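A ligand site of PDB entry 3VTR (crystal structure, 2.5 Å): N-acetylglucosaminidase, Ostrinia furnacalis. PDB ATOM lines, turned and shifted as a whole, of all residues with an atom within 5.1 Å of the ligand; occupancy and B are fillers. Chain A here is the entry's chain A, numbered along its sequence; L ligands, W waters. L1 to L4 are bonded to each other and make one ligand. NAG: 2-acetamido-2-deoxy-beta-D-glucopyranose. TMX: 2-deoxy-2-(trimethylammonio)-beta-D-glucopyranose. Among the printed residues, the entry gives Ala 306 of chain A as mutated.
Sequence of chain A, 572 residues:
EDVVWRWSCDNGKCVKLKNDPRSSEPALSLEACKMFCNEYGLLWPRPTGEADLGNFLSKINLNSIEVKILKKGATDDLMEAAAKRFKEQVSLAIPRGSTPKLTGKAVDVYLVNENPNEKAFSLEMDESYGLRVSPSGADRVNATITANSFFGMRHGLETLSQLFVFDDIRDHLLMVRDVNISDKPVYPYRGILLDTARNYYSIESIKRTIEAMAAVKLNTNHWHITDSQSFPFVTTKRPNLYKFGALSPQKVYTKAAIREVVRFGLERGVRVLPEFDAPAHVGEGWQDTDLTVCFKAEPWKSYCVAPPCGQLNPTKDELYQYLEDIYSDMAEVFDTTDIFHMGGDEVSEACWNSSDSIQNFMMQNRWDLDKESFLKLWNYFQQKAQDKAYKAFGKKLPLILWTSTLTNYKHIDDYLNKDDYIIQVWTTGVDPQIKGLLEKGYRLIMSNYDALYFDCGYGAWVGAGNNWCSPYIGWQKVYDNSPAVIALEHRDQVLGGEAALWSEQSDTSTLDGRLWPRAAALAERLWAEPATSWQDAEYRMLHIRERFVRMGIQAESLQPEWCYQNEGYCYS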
ATOM      1  N   ASP A 195       7.922  16.657 -13.531  1.00  0.00           N
ATOM      2  CA  ASP A 195       6.866  15.667 -13.775  1.00  0.00           C
ATOM      3  C   ASP A 195       7.479  14.261 -13.624  1.00  0.00           C
ATOM      4  O   ASP A 195       8.263  13.840 -14.458  1.00  0.00           O
ATOM      5  CB  ASP A 195       6.274  15.945 -15.163  1.00  0.00           C
ATOM      6  CG  ASP A 195       5.440  14.803 -15.728  1.00  0.00           C
ATOM      7  OD1 ASP A 195       5.071  14.901 -16.920  1.00  0.00           O
ATOM      8  OD2 ASP A 195       5.138  13.812 -15.015  1.00  0.00           O
ATOM      9  N   ARG A 198       4.798  11.099 -16.092  1.00  0.00           N
ATOM     10  CA  ARG A 198       4.934  10.750 -17.498  1.00  0.00           C
ATOM     11  C   ARG A 198       6.158   9.849 -17.753  1.00  0.00           C
ATOM     12  O   ARG A 198       6.185   9.087 -18.719  1.00  0.00           O
ATOM     13  CB  ARG A 198       4.961  12.001 -18.371  1.00  0.00           C
ATOM     14  CG  ARG A 198       3.595  12.454 -18.882  1.00  0.00           C
ATOM     15  CD  ARG A 198       2.614  12.833 -17.763  1.00  0.00           C
ATOM     16  NE  ARG A 198       1.444  13.504 -18.317  1.00  0.00           N
ATOM     17  CZ  ARG A 198       1.350  14.811 -18.523  1.00  0.00           C
ATOM     18  NH1 ARG A 198       2.366  15.615 -18.203  1.00  0.00           N
ATOM     19  NH2 ARG A 198       0.237  15.323 -19.048  1.00  0.00           N
ATOM     20  N   ASP A 227      -0.054  11.509 -12.708  1.00  0.00           N
ATOM     21  CA  ASP A 227      -0.781  11.883 -13.902  1.00  0.00           C
ATOM     22  C   ASP A 227      -1.490  10.636 -14.408  1.00  0.00           C
ATOM     23  O   ASP A 227      -1.537   9.632 -13.689  1.00  0.00           O
ATOM     24  CB  ASP A 227       0.144  12.474 -14.971  1.00  0.00           C
ATOM     25  CG  ASP A 227      -0.543  13.504 -15.834  1.00  0.00           C
ATOM     26  OD1 ASP A 227      -1.455  13.135 -16.613  1.00  0.00           O
ATOM     27  OD2 ASP A 227      -0.175  14.698 -15.743  1.00  0.00           O
ATOM     28  N   HIS A 281      -6.194  14.364 -15.729  1.00  0.00           N
ATOM     29  CA  HIS A 281      -4.861  13.771 -15.544  1.00  0.00           C
ATOM     30  C   HIS A 281      -4.815  12.697 -14.462  1.00  0.00           C
ATOM     31  O   HIS A 281      -3.938  12.699 -13.593  1.00  0.00           O
ATOM     32  CB  HIS A 281      -3.821  14.859 -15.298  1.00  0.00           C
ATOM     33  CG  HIS A 281      -3.565  15.704 -16.494  1.00  0.00           C
ATOM     34  ND1 HIS A 281      -2.645  15.364 -17.469  1.00  0.00           N
ATOM     35  CD2 HIS A 281      -4.156  16.849 -16.917  1.00  0.00           C
ATOM     36  CE1 HIS A 281      -2.661  16.284 -18.411  1.00  0.00           C
ATOM     37  NE2 HIS A 281      -3.561  17.195 -18.109  1.00  0.00           N
ATOM     38  N   TRP A 300      -8.454   8.779 -28.756  1.00  0.00           N
ATOM     39  CA  TRP A 300      -8.093   9.703 -27.671  1.00  0.00           C
ATOM     40  C   TRP A 300      -8.311  11.167 -28.053  1.00  0.00           C
ATOM     41  O   TRP A 300      -8.698  11.975 -27.215  1.00  0.00           O
ATOM     42  CB  TRP A 300      -6.655   9.482 -27.171  1.00  0.00           C
ATOM     43  CG  TRP A 300      -5.576   9.818 -28.158  1.00  0.00           C
ATOM     44  CD1 TRP A 300      -4.944   8.956 -28.998  1.00  0.00           C
ATOM     45  CD2 TRP A 300      -4.995  11.112 -28.407  1.00  0.00           C
ATOM     46  NE1 TRP A 300      -4.006   9.625 -29.753  1.00  0.00           N
ATOM     47  CE2 TRP A 300      -4.025  10.951 -29.405  1.00  0.00           C
ATOM     48  CE3 TRP A 300      -5.215  12.396 -27.877  1.00  0.00           C
ATOM     49  CZ2 TRP A 300      -3.262  12.010 -29.907  1.00  0.00           C
ATOM     50  CZ3 TRP A 300      -4.455  13.453 -28.365  1.00  0.00           C
ATOM     51  CH2 TRP A 300      -3.494  13.252 -29.371  1.00  0.00           C
ATOM     52  N   LYS A 301      -8.094  11.481 -29.330  1.00  0.00           N
ATOM     53  CA  LYS A 301      -8.198  12.848 -29.823  1.00  0.00           C
ATOM     54  C   LYS A 301      -9.578  13.460 -29.577  1.00  0.00           C
ATOM     55  O   LYS A 301      -9.706  14.682 -29.494  1.00  0.00           O
ATOM     56  CB  LYS A 301      -7.830  12.928 -31.308  1.00  0.00           C
ATOM     57  CG  LYS A 301      -7.561  14.338 -31.819  1.00  0.00           C
ATOM     58  CD  LYS A 301      -6.585  15.096 -30.921  1.00  0.00           C
ATOM     59  CE  LYS A 301      -6.550  16.592 -31.248  1.00  0.00           C
ATOM     60  NZ  LYS A 301      -5.871  16.878 -32.553  1.00  0.00           N
ATOM     61  N   CYS A 304      -9.344  13.736 -24.787  1.00  0.00           N
ATOM     62  CA  CYS A 304      -8.324  14.579 -24.161  1.00  0.00           C
ATOM     63  C   CYS A 304      -7.311  15.103 -25.182  1.00  0.00           C
ATOM     64  O   CYS A 304      -7.390  14.778 -26.371  1.00  0.00           O
ATOM     65  CB  CYS A 304      -7.644  13.802 -23.025  1.00  0.00           C
ATOM     66  SG  CYS A 304      -6.841  12.260 -23.587  1.00  0.00           S
ATOM     67  N   VAL A 305      -6.381  15.934 -24.725  1.00  0.00           N
ATOM     68  CA  VAL A 305      -5.375  16.553 -25.595  1.00  0.00           C
ATOM     69  C   VAL A 305      -4.096  15.727 -25.740  1.00  0.00           C
ATOM     70  O   VAL A 305      -3.176  16.116 -26.448  1.00  0.00           O
ATOM     71  CB  VAL A 305      -5.036  18.001 -25.170  1.00  0.00           C
ATOM     72  CG1 VAL A 305      -6.295  18.870 -25.118  1.00  0.00           C
ATOM     73  CG2 VAL A 305      -4.294  18.029 -23.839  1.00  0.00           C
ATOM     74  N   ALA A 306      -4.047  14.584 -25.039  1.00  0.00           N
ATOM     75  CA  ALA A 306      -2.905  13.673 -25.102  1.00  0.00           C
ATOM     76  C   ALA A 306      -3.238  12.366 -24.395  1.00  0.00           C
ATOM     77  O   ALA A 306      -3.846  12.377 -23.333  1.00  0.00           O
ATOM     78  CB  ALA A 306      -1.654  14.309 -24.487  1.00  0.00           C
ATOM     79  N   PRO A 307      -2.825  11.232 -24.992  1.00  0.00           N
ATOM     80  CA  PRO A 307      -3.095   9.916 -24.418  1.00  0.00           C
ATOM     81  C   PRO A 307      -2.172   9.595 -23.237  1.00  0.00           C
ATOM     82  O   PRO A 307      -1.048  10.098 -23.196  1.00  0.00           O
ATOM     83  CB  PRO A 307      -2.829   8.969 -25.588  1.00  0.00           C
ATOM     84  CG  PRO A 307      -1.794   9.664 -26.390  1.00  0.00           C
ATOM     85  CD  PRO A 307      -2.047  11.139 -26.245  1.00  0.00           C
ATOM     86  N   ASP A 345      -5.538  21.297 -14.630  1.00  0.00           N
ATOM     87  CA  ASP A 345      -5.307  21.328 -16.080  1.00  0.00           C
ATOM     88  C   ASP A 345      -6.627  21.099 -16.789  1.00  0.00           C
ATOM     89  O   ASP A 345      -7.503  20.408 -16.249  1.00  0.00           O
ATOM     90  CB  ASP A 345      -4.340  20.224 -16.502  1.00  0.00           C
ATOM     91  CG  ASP A 345      -3.107  20.163 -15.632  1.00  0.00           C
ATOM     92  OD1 ASP A 345      -2.860  21.109 -14.864  1.00  0.00           O
ATOM     93  OD2 ASP A 345      -2.378  19.161 -15.737  1.00  0.00           O
ATOM     94  N   TRP A 426       0.568  29.261 -17.558  1.00  0.00           N
ATOM     95  CA  TRP A 426       1.276  28.608 -18.660  1.00  0.00           C
ATOM     96  C   TRP A 426       0.926  29.183 -20.033  1.00  0.00           C
ATOM     97  O   TRP A 426       1.356  28.643 -21.052  1.00  0.00           O
ATOM     98  CB  TRP A 426       1.040  27.093 -18.646  1.00  0.00           C
ATOM     99  CG  TRP A 426      -0.357  26.683 -18.972  1.00  0.00           C
ATOM    100  CD1 TRP A 426      -1.466  26.894 -18.204  1.00  0.00           C
ATOM    101  CD2 TRP A 426      -0.809  25.993 -20.156  1.00  0.00           C
ATOM    102  NE1 TRP A 426      -2.580  26.394 -18.828  1.00  0.00           N
ATOM    103  CE2 TRP A 426      -2.208  25.836 -20.025  1.00  0.00           C
ATOM    104  CE3 TRP A 426      -0.164  25.498 -21.296  1.00  0.00           C
ATOM    105  CZ2 TRP A 426      -2.982  25.190 -21.007  1.00  0.00           C
ATOM    106  CZ3 TRP A 426      -0.935  24.872 -22.267  1.00  0.00           C
ATOM    107  CH2 TRP A 426      -2.324  24.725 -22.117  1.00  0.00           C
ATOM    108  N   TYR A 453       8.851  26.450 -20.814  1.00  0.00           N
ATOM    109  CA  TYR A 453       8.629  25.006 -20.970  1.00  0.00           C
ATOM    110  C   TYR A 453       9.885  24.329 -21.495  1.00  0.00           C
ATOM    111  O   TYR A 453      10.249  24.475 -22.657  1.00  0.00           O
ATOM    112  CB  TYR A 453       7.433  24.730 -21.876  1.00  0.00           C
ATOM    113  CG  TYR A 453       6.117  24.649 -21.144  1.00  0.00           C
ATOM    114  CD1 TYR A 453       5.116  23.766 -21.559  1.00  0.00           C
ATOM    115  CD2 TYR A 453       5.868  25.452 -20.026  1.00  0.00           C
ATOM    116  CE1 TYR A 453       3.902  23.692 -20.890  1.00  0.00           C
ATOM    117  CE2 TYR A 453       4.673  25.380 -19.346  1.00  0.00           C
ATOM    118  CZ  TYR A 453       3.691  24.501 -19.785  1.00  0.00           C
ATOM    119  OH  TYR A 453       2.508  24.449 -19.099  1.00  0.00           O
ATOM    120  N   ASP A 455      10.634  21.237 -21.991  1.00  0.00           N
ATOM    121  CA  ASP A 455      10.422  20.015 -22.781  1.00  0.00           C
ATOM    122  C   ASP A 455      10.262  20.310 -24.271  1.00  0.00           C
ATOM    123  O   ASP A 455      10.347  19.397 -25.091  1.00  0.00           O
ATOM    124  CB  ASP A 455       9.178  19.278 -22.273  1.00  0.00           C
ATOM    125  CG  ASP A 455       7.927  20.162 -22.261  1.00  0.00           C
ATOM    126  OD1 ASP A 455       7.999  21.297 -21.742  1.00  0.00           O
ATOM    127  OD2 ASP A 455       6.885  19.709 -22.775  1.00  0.00           O
ATOM    128  N   TRP A 461       6.395  12.891 -29.909  1.00  0.00           N
ATOM    129  CA  TRP A 461       6.223  11.606 -29.242  1.00  0.00           C
ATOM    130  C   TRP A 461       4.958  10.891 -29.710  1.00  0.00           C
ATOM    131  O   TRP A 461       4.722   9.725 -29.363  1.00  0.00           O
ATOM    132  CB  TRP A 461       6.313  11.703 -27.715  1.00  0.00           C
ATOM    133  CG  TRP A 461       5.222  12.471 -27.030  1.00  0.00           C
ATOM    134  CD1 TRP A 461       5.193  13.808 -26.793  1.00  0.00           C
ATOM    135  CD2 TRP A 461       4.040  11.933 -26.424  1.00  0.00           C
ATOM    136  NE1 TRP A 461       4.055  14.145 -26.096  1.00  0.00           N
ATOM    137  CE2 TRP A 461       3.326  13.019 -25.865  1.00  0.00           C
ATOM    138  CE3 TRP A 461       3.501  10.639 -26.318  1.00  0.00           C
ATOM    139  CZ2 TRP A 461       2.105  12.854 -25.196  1.00  0.00           C
ATOM    140  CZ3 TRP A 461       2.275  10.474 -25.657  1.00  0.00           C
ATOM    141  CH2 TRP A 461       1.599  11.575 -25.110  1.00  0.00           C
ATOM    142  N   VAL A 462       4.149  11.597 -30.498  1.00  0.00           N
ATOM    143  CA  VAL A 462       3.075  10.988 -31.281  1.00  0.00           C
ATOM    144  C   VAL A 462       3.157  11.526 -32.712  1.00  0.00           C
ATOM    145  O   VAL A 462       3.249  12.733 -32.932  1.00  0.00           O
ATOM    146  CB  VAL A 462       1.651  11.232 -30.669  1.00  0.00           C
ATOM    147  CG1 VAL A 462       1.516  10.553 -29.305  1.00  0.00           C
ATOM    148  CG2 VAL A 462       1.310  12.723 -30.586  1.00  0.00           C
ATOM    149  N   TRP A 468       4.826  19.570 -29.453  1.00  0.00           N
ATOM    150  CA  TRP A 468       3.806  20.630 -29.613  1.00  0.00           C
ATOM    151  C   TRP A 468       4.310  22.073 -29.443  1.00  0.00           C
ATOM    152  O   TRP A 468       3.938  22.946 -30.225  1.00  0.00           O
ATOM    153  CB  TRP A 468       2.578  20.370 -28.731  1.00  0.00           C
ATOM    154  CG  TRP A 468       2.730  20.820 -27.311  1.00  0.00           C
ATOM    155  CD1 TRP A 468       3.300  20.124 -26.292  1.00  0.00           C
ATOM    156  CD2 TRP A 468       2.324  22.082 -26.761  1.00  0.00           C
ATOM    157  NE1 TRP A 468       3.273  20.866 -25.138  1.00  0.00           N
ATOM    158  CE2 TRP A 468       2.675  22.074 -25.400  1.00  0.00           C
ATOM    159  CE3 TRP A 468       1.702  23.225 -27.293  1.00  0.00           C
ATOM    160  CZ2 TRP A 468       2.429  23.158 -24.544  1.00  0.00           C
ATOM    161  CZ3 TRP A 468       1.446  24.300 -26.455  1.00  0.00           C
ATOM    162  CH2 TRP A 468       1.805  24.262 -25.089  1.00  0.00           C
ATOM    163  N   CYS A 469       5.140  22.307 -28.430  1.00  0.00           N
ATOM    164  CA  CYS A 469       5.550  23.670 -28.087  1.00  0.00           C
ATOM    165  C   CYS A 469       6.930  24.063 -28.645  1.00  0.00           C
ATOM    166  O   CYS A 469       7.515  25.064 -28.238  1.00  0.00           O
ATOM    167  CB  CYS A 469       5.481  23.873 -26.576  1.00  0.00           C
ATOM    168  SG  CYS A 469       6.537  22.771 -25.615  1.00  0.00           S
ATOM    169  N   TRP A 502       8.048  18.986 -18.285  1.00  0.00           N
ATOM    170  CA  TRP A 502       7.098  17.906 -18.517  1.00  0.00           C
ATOM    171  C   TRP A 502       7.864  16.724 -19.076  1.00  0.00           C
ATOM    172  O   TRP A 502       8.810  16.891 -19.845  1.00  0.00           O
ATOM    173  CB  TRP A 502       5.988  18.372 -19.457  1.00  0.00           C
ATOM    174  CG  TRP A 502       5.268  19.535 -18.868  1.00  0.00           C
ATOM    175  CD1 TRP A 502       5.405  20.842 -19.218  1.00  0.00           C
ATOM    176  CD2 TRP A 502       4.318  19.498 -17.797  1.00  0.00           C
ATOM    177  NE1 TRP A 502       4.595  21.631 -18.437  1.00  0.00           N
ATOM    178  CE2 TRP A 502       3.910  20.824 -17.561  1.00  0.00           C
ATOM    179  CE3 TRP A 502       3.763  18.473 -17.023  1.00  0.00           C
ATOM    180  CZ2 TRP A 502       2.978  21.161 -16.568  1.00  0.00           C
ATOM    181  CZ3 TRP A 502       2.835  18.802 -16.044  1.00  0.00           C
ATOM    182  CH2 TRP A 502       2.452  20.133 -15.824  1.00  0.00           C
ATOM    183  N   GLU A 504       7.019  13.698 -20.758  1.00  0.00           N
ATOM    184  CA  GLU A 504       6.619  12.791 -21.842  1.00  0.00           C
ATOM    185  C   GLU A 504       7.865  12.286 -22.566  1.00  0.00           C
ATOM    186  O   GLU A 504       7.954  11.121 -22.927  1.00  0.00           O
ATOM    187  CB  GLU A 504       5.702  13.487 -22.846  1.00  0.00           C
ATOM    188  CG  GLU A 504       4.302  13.815 -22.328  1.00  0.00           C
ATOM    189  CD  GLU A 504       4.230  15.170 -21.652  1.00  0.00           C
ATOM    190  OE1 GLU A 504       5.283  15.755 -21.316  1.00  0.00           O
ATOM    191  OE2 GLU A 504       3.102  15.651 -21.438  1.00  0.00           O
HETATM  192  C1  NAG L   1      -4.883  19.220 -34.874  1.00  0.00           C
HETATM  193  C2  NAG L   1      -3.396  18.869 -34.716  1.00  0.00           C
HETATM  194  C3  NAG L   1      -2.614  20.086 -34.234  1.00  0.00           C
HETATM  195  C4  NAG L   1      -3.448  21.070 -33.417  1.00  0.00           C
HETATM  196  C5  NAG L   1      -4.751  21.465 -34.075  1.00  0.00           C
HETATM  197  C6  NAG L   1      -4.646  22.918 -34.494  1.00  0.00           C
HETATM  198  C7  NAG L   1      -3.022  16.558 -34.111  1.00  0.00           C
HETATM  199  C8  NAG L   1      -2.886  15.507 -33.049  1.00  0.00           C
HETATM  200  N2  NAG L   1      -3.265  17.815 -33.722  1.00  0.00           N
HETATM  201  O1  NAG L   1      -5.449  18.424 -35.945  1.00  0.00           O
HETATM  202  O3  NAG L   1      -2.077  20.783 -35.364  1.00  0.00           O
HETATM  203  O4  NAG L   1      -3.764  20.515 -32.159  1.00  0.00           O
HETATM  204  O5  NAG L   1      -4.999  20.619 -35.204  1.00  0.00           O
HETATM  205  O6  NAG L   1      -5.845  23.322 -35.229  1.00  0.00           O
HETATM  206  O7  NAG L   1      -2.908  16.274 -35.301  1.00  0.00           O
HETATM  207  C1  NAG L   2      -2.590  20.173 -31.465  1.00  0.00           C
HETATM  208  C2  NAG L   2      -2.416  21.273 -30.422  1.00  0.00           C
HETATM  209  C3  NAG L   2      -1.503  20.855 -29.286  1.00  0.00           C
HETATM  210  C4  NAG L   2      -1.860  19.474 -28.755  1.00  0.00           C
HETATM  211  C5  NAG L   2      -2.007  18.436 -29.872  1.00  0.00           C
HETATM  212  C6  NAG L   2      -2.570  17.122 -29.328  1.00  0.00           C
HETATM  213  C7  NAG L   2      -2.264  23.566 -31.259  1.00  0.00           C
HETATM  214  C8  NAG L   2      -1.425  24.612 -31.950  1.00  0.00           C
HETATM  215  N2  NAG L   2      -1.697  22.374 -31.083  1.00  0.00           N
HETATM  216  O3  NAG L   2      -1.645  21.809 -28.241  1.00  0.00           O
HETATM  217  O4  NAG L   2      -0.755  19.095 -27.973  1.00  0.00           O
HETATM  218  O5  NAG L   2      -2.884  18.896 -30.899  1.00  0.00           O
HETATM  219  O6  NAG L   2      -3.987  17.270 -29.043  1.00  0.00           O
HETATM  220  O7  NAG L   2      -3.407  23.818 -30.904  1.00  0.00           O
HETATM  221  C1  NAG L   3      -1.004  19.099 -26.581  1.00  0.00           C
HETATM  222  C2  NAG L   3       0.112  18.256 -25.989  1.00  0.00           C
HETATM  223  C3  NAG L   3      -0.024  18.269 -24.467  1.00  0.00           C
HETATM  224  C4  NAG L   3      -0.075  19.693 -23.930  1.00  0.00           C
HETATM  225  C5  NAG L   3      -1.126  20.528 -24.669  1.00  0.00           C
HETATM  226  C6  NAG L   3      -1.069  22.001 -24.291  1.00  0.00           C
HETATM  227  C7  NAG L   3       0.534  16.240 -27.405  1.00  0.00           C
HETATM  228  C8  NAG L   3       1.658  16.943 -28.098  1.00  0.00           C
HETATM  229  N2  NAG L   3      -0.140  16.892 -26.442  1.00  0.00           N
HETATM  230  O3  NAG L   3       1.065  17.536 -23.889  1.00  0.00           O
HETATM  231  O4  NAG L   3      -0.417  19.547 -22.558  1.00  0.00           O
HETATM  232  O5  NAG L   3      -0.916  20.430 -26.075  1.00  0.00           O
HETATM  233  O6  NAG L   3      -2.187  22.671 -24.877  1.00  0.00           O
HETATM  234  O7  NAG L   3       0.251  15.089 -27.712  1.00  0.00           O
HETATM  235  C1  TMX L   4       0.191  20.455 -21.638  1.00  0.00           C
HETATM  236  C2  TMX L   4      -0.218  19.993 -20.213  1.00  0.00           C
HETATM  237  N2  TMX L   4      -0.487  21.151 -19.316  1.00  0.00           N
HETATM  238  C3  TMX L   4       0.757  18.972 -19.612  1.00  0.00           C
HETATM  239  O3  TMX L   4       0.024  17.855 -19.096  1.00  0.00           O
HETATM  240  C4  TMX L   4       1.762  18.495 -20.644  1.00  0.00           C
HETATM  241  O4  TMX L   4       2.677  17.586 -20.012  1.00  0.00           O
HETATM  242  C5  TMX L   4       2.500  19.706 -21.183  1.00  0.00           C
HETATM  243  O5  TMX L   4       1.605  20.603 -21.862  1.00  0.00           O
HETATM  244  C6  TMX L   4       3.594  19.283 -22.150  1.00  0.00           C
HETATM  245  O6  TMX L   4       4.202  20.463 -22.716  1.00  0.00           O
HETATM  246  C7  TMX L   4      -1.612  21.947 -19.857  1.00  0.00           C
HETATM  247  C8  TMX L   4       0.654  22.065 -19.128  1.00  0.00           C
HETATM  248  C9  TMX L   4      -0.915  20.667 -17.986  1.00  0.00           C
HETATM  249  O   HOH W   1       1.201  22.625 -31.412  1.00  0.00           O
HETATM  250  O   HOH W   2      -2.124  16.346 -21.345  1.00  0.00           O
HETATM  251  O   HOH W   3      -2.125  25.610 -26.080  1.00  0.00           O
HETATM  252  O   HOH W   4      -0.503  17.428 -16.618  1.00  0.00           O
HETATM  253  O   HOH W   5      -3.475  19.266 -20.894  1.00  0.00           O
HETATM  254  O   HOH W   6       4.427  17.115 -27.926  1.00  0.00           O
HETATM  255  O   HOH W   7       3.489  16.647 -25.007  1.00  0.00           O
HETATM  256  O   HOH W   8       0.736  15.232 -22.377  1.00  0.00           O
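Water W4 lies within hydrogen-bond range of O3 of TMX L4 (2.6 Å), OD2 of Asp 345 (2.7 Å), OD2 of Asp 227 (2.9 Å), ND1 of His 281 (3.1 Å) and NH2 of Arg 198 (3.3 Å).
Water W8 lies within hydrogen-bond range of the side-chain carboxylate of Glu 504 (2.6 Å), an oxygen (O3) of NAG L3 (2.8 Å) and the guanidinium group of Arg 198 (3.4 Å).
Water W7 bridges NE1 of Trp 461 (2.8 Å) and O3 of NAG L3 (2.8 Å).
Water W1 bridges N2 of NAG L2 (2.9 Å) and O of Trp 468 (3.0 Å).
Water W5 lies within hydrogen-bond range of a ring nitrogen (NE2) of His 281 (3.5 Å) and an oxygen (O4) of NAG L3 (3.5 Å).
Water W2 lies within hydrogen-bond range of NH2 of Arg 198 and O3 of TMX L4.
The side-chain carboxylate (OD1) of Asp 227 sits at hydrogen-bond distance from a ring nitrogen (ND1) of His 281 (2.7 Å).
OE2 of Glu 504 is in salt-bridge range of NH1 of Arg 198, 3.3 Å away.
NH1 of Arg 198 lies within salt-bridge range of OD1 of Asp 195, 3.1 Å away.
The guanidinium group (NE) of Arg 198 lies within salt-bridge range of the side-chain carboxylate (OD2) of Asp 227 (3.3 Å).
ND1 of His 281 sits close to NH2 of Arg 198 (3.3 Å).
OD2 of Asp 345 lies close to NE2 of His 281 (3.3 Å).
O6 of NAG L2 is in hydrogen-bond range of O of Val 305.
The guanidinium group of Arg 198 lies within hydrogen-bond range of an oxygen (O3) of TMX L4 (2.5 Å).
An oxygen (O6) of TMX L4 sits at hydrogen-bond distance from the side-chain carboxylate (OD2) of Asp 455, 2.8 Å away.
The indole nitrogen (NE1) of Trp 468 is in hydrogen-bond range of an oxygen (O6) of TMX L4.
The side-chain carboxylate of Glu 504 is in hydrogen-bond range of an oxygen (O4) of TMX L4, at 2.4 Å.
The side-chain amino group of Lys 301 sits close to a nitrogen (N2) of NAG L1 (3.0 Å).
Residues that only touch the ligand: Tyr 453, Asp 345, His 281, Trp 502, Trp 426, Ala 306, Trp 461, Val 462 and Trp 300.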
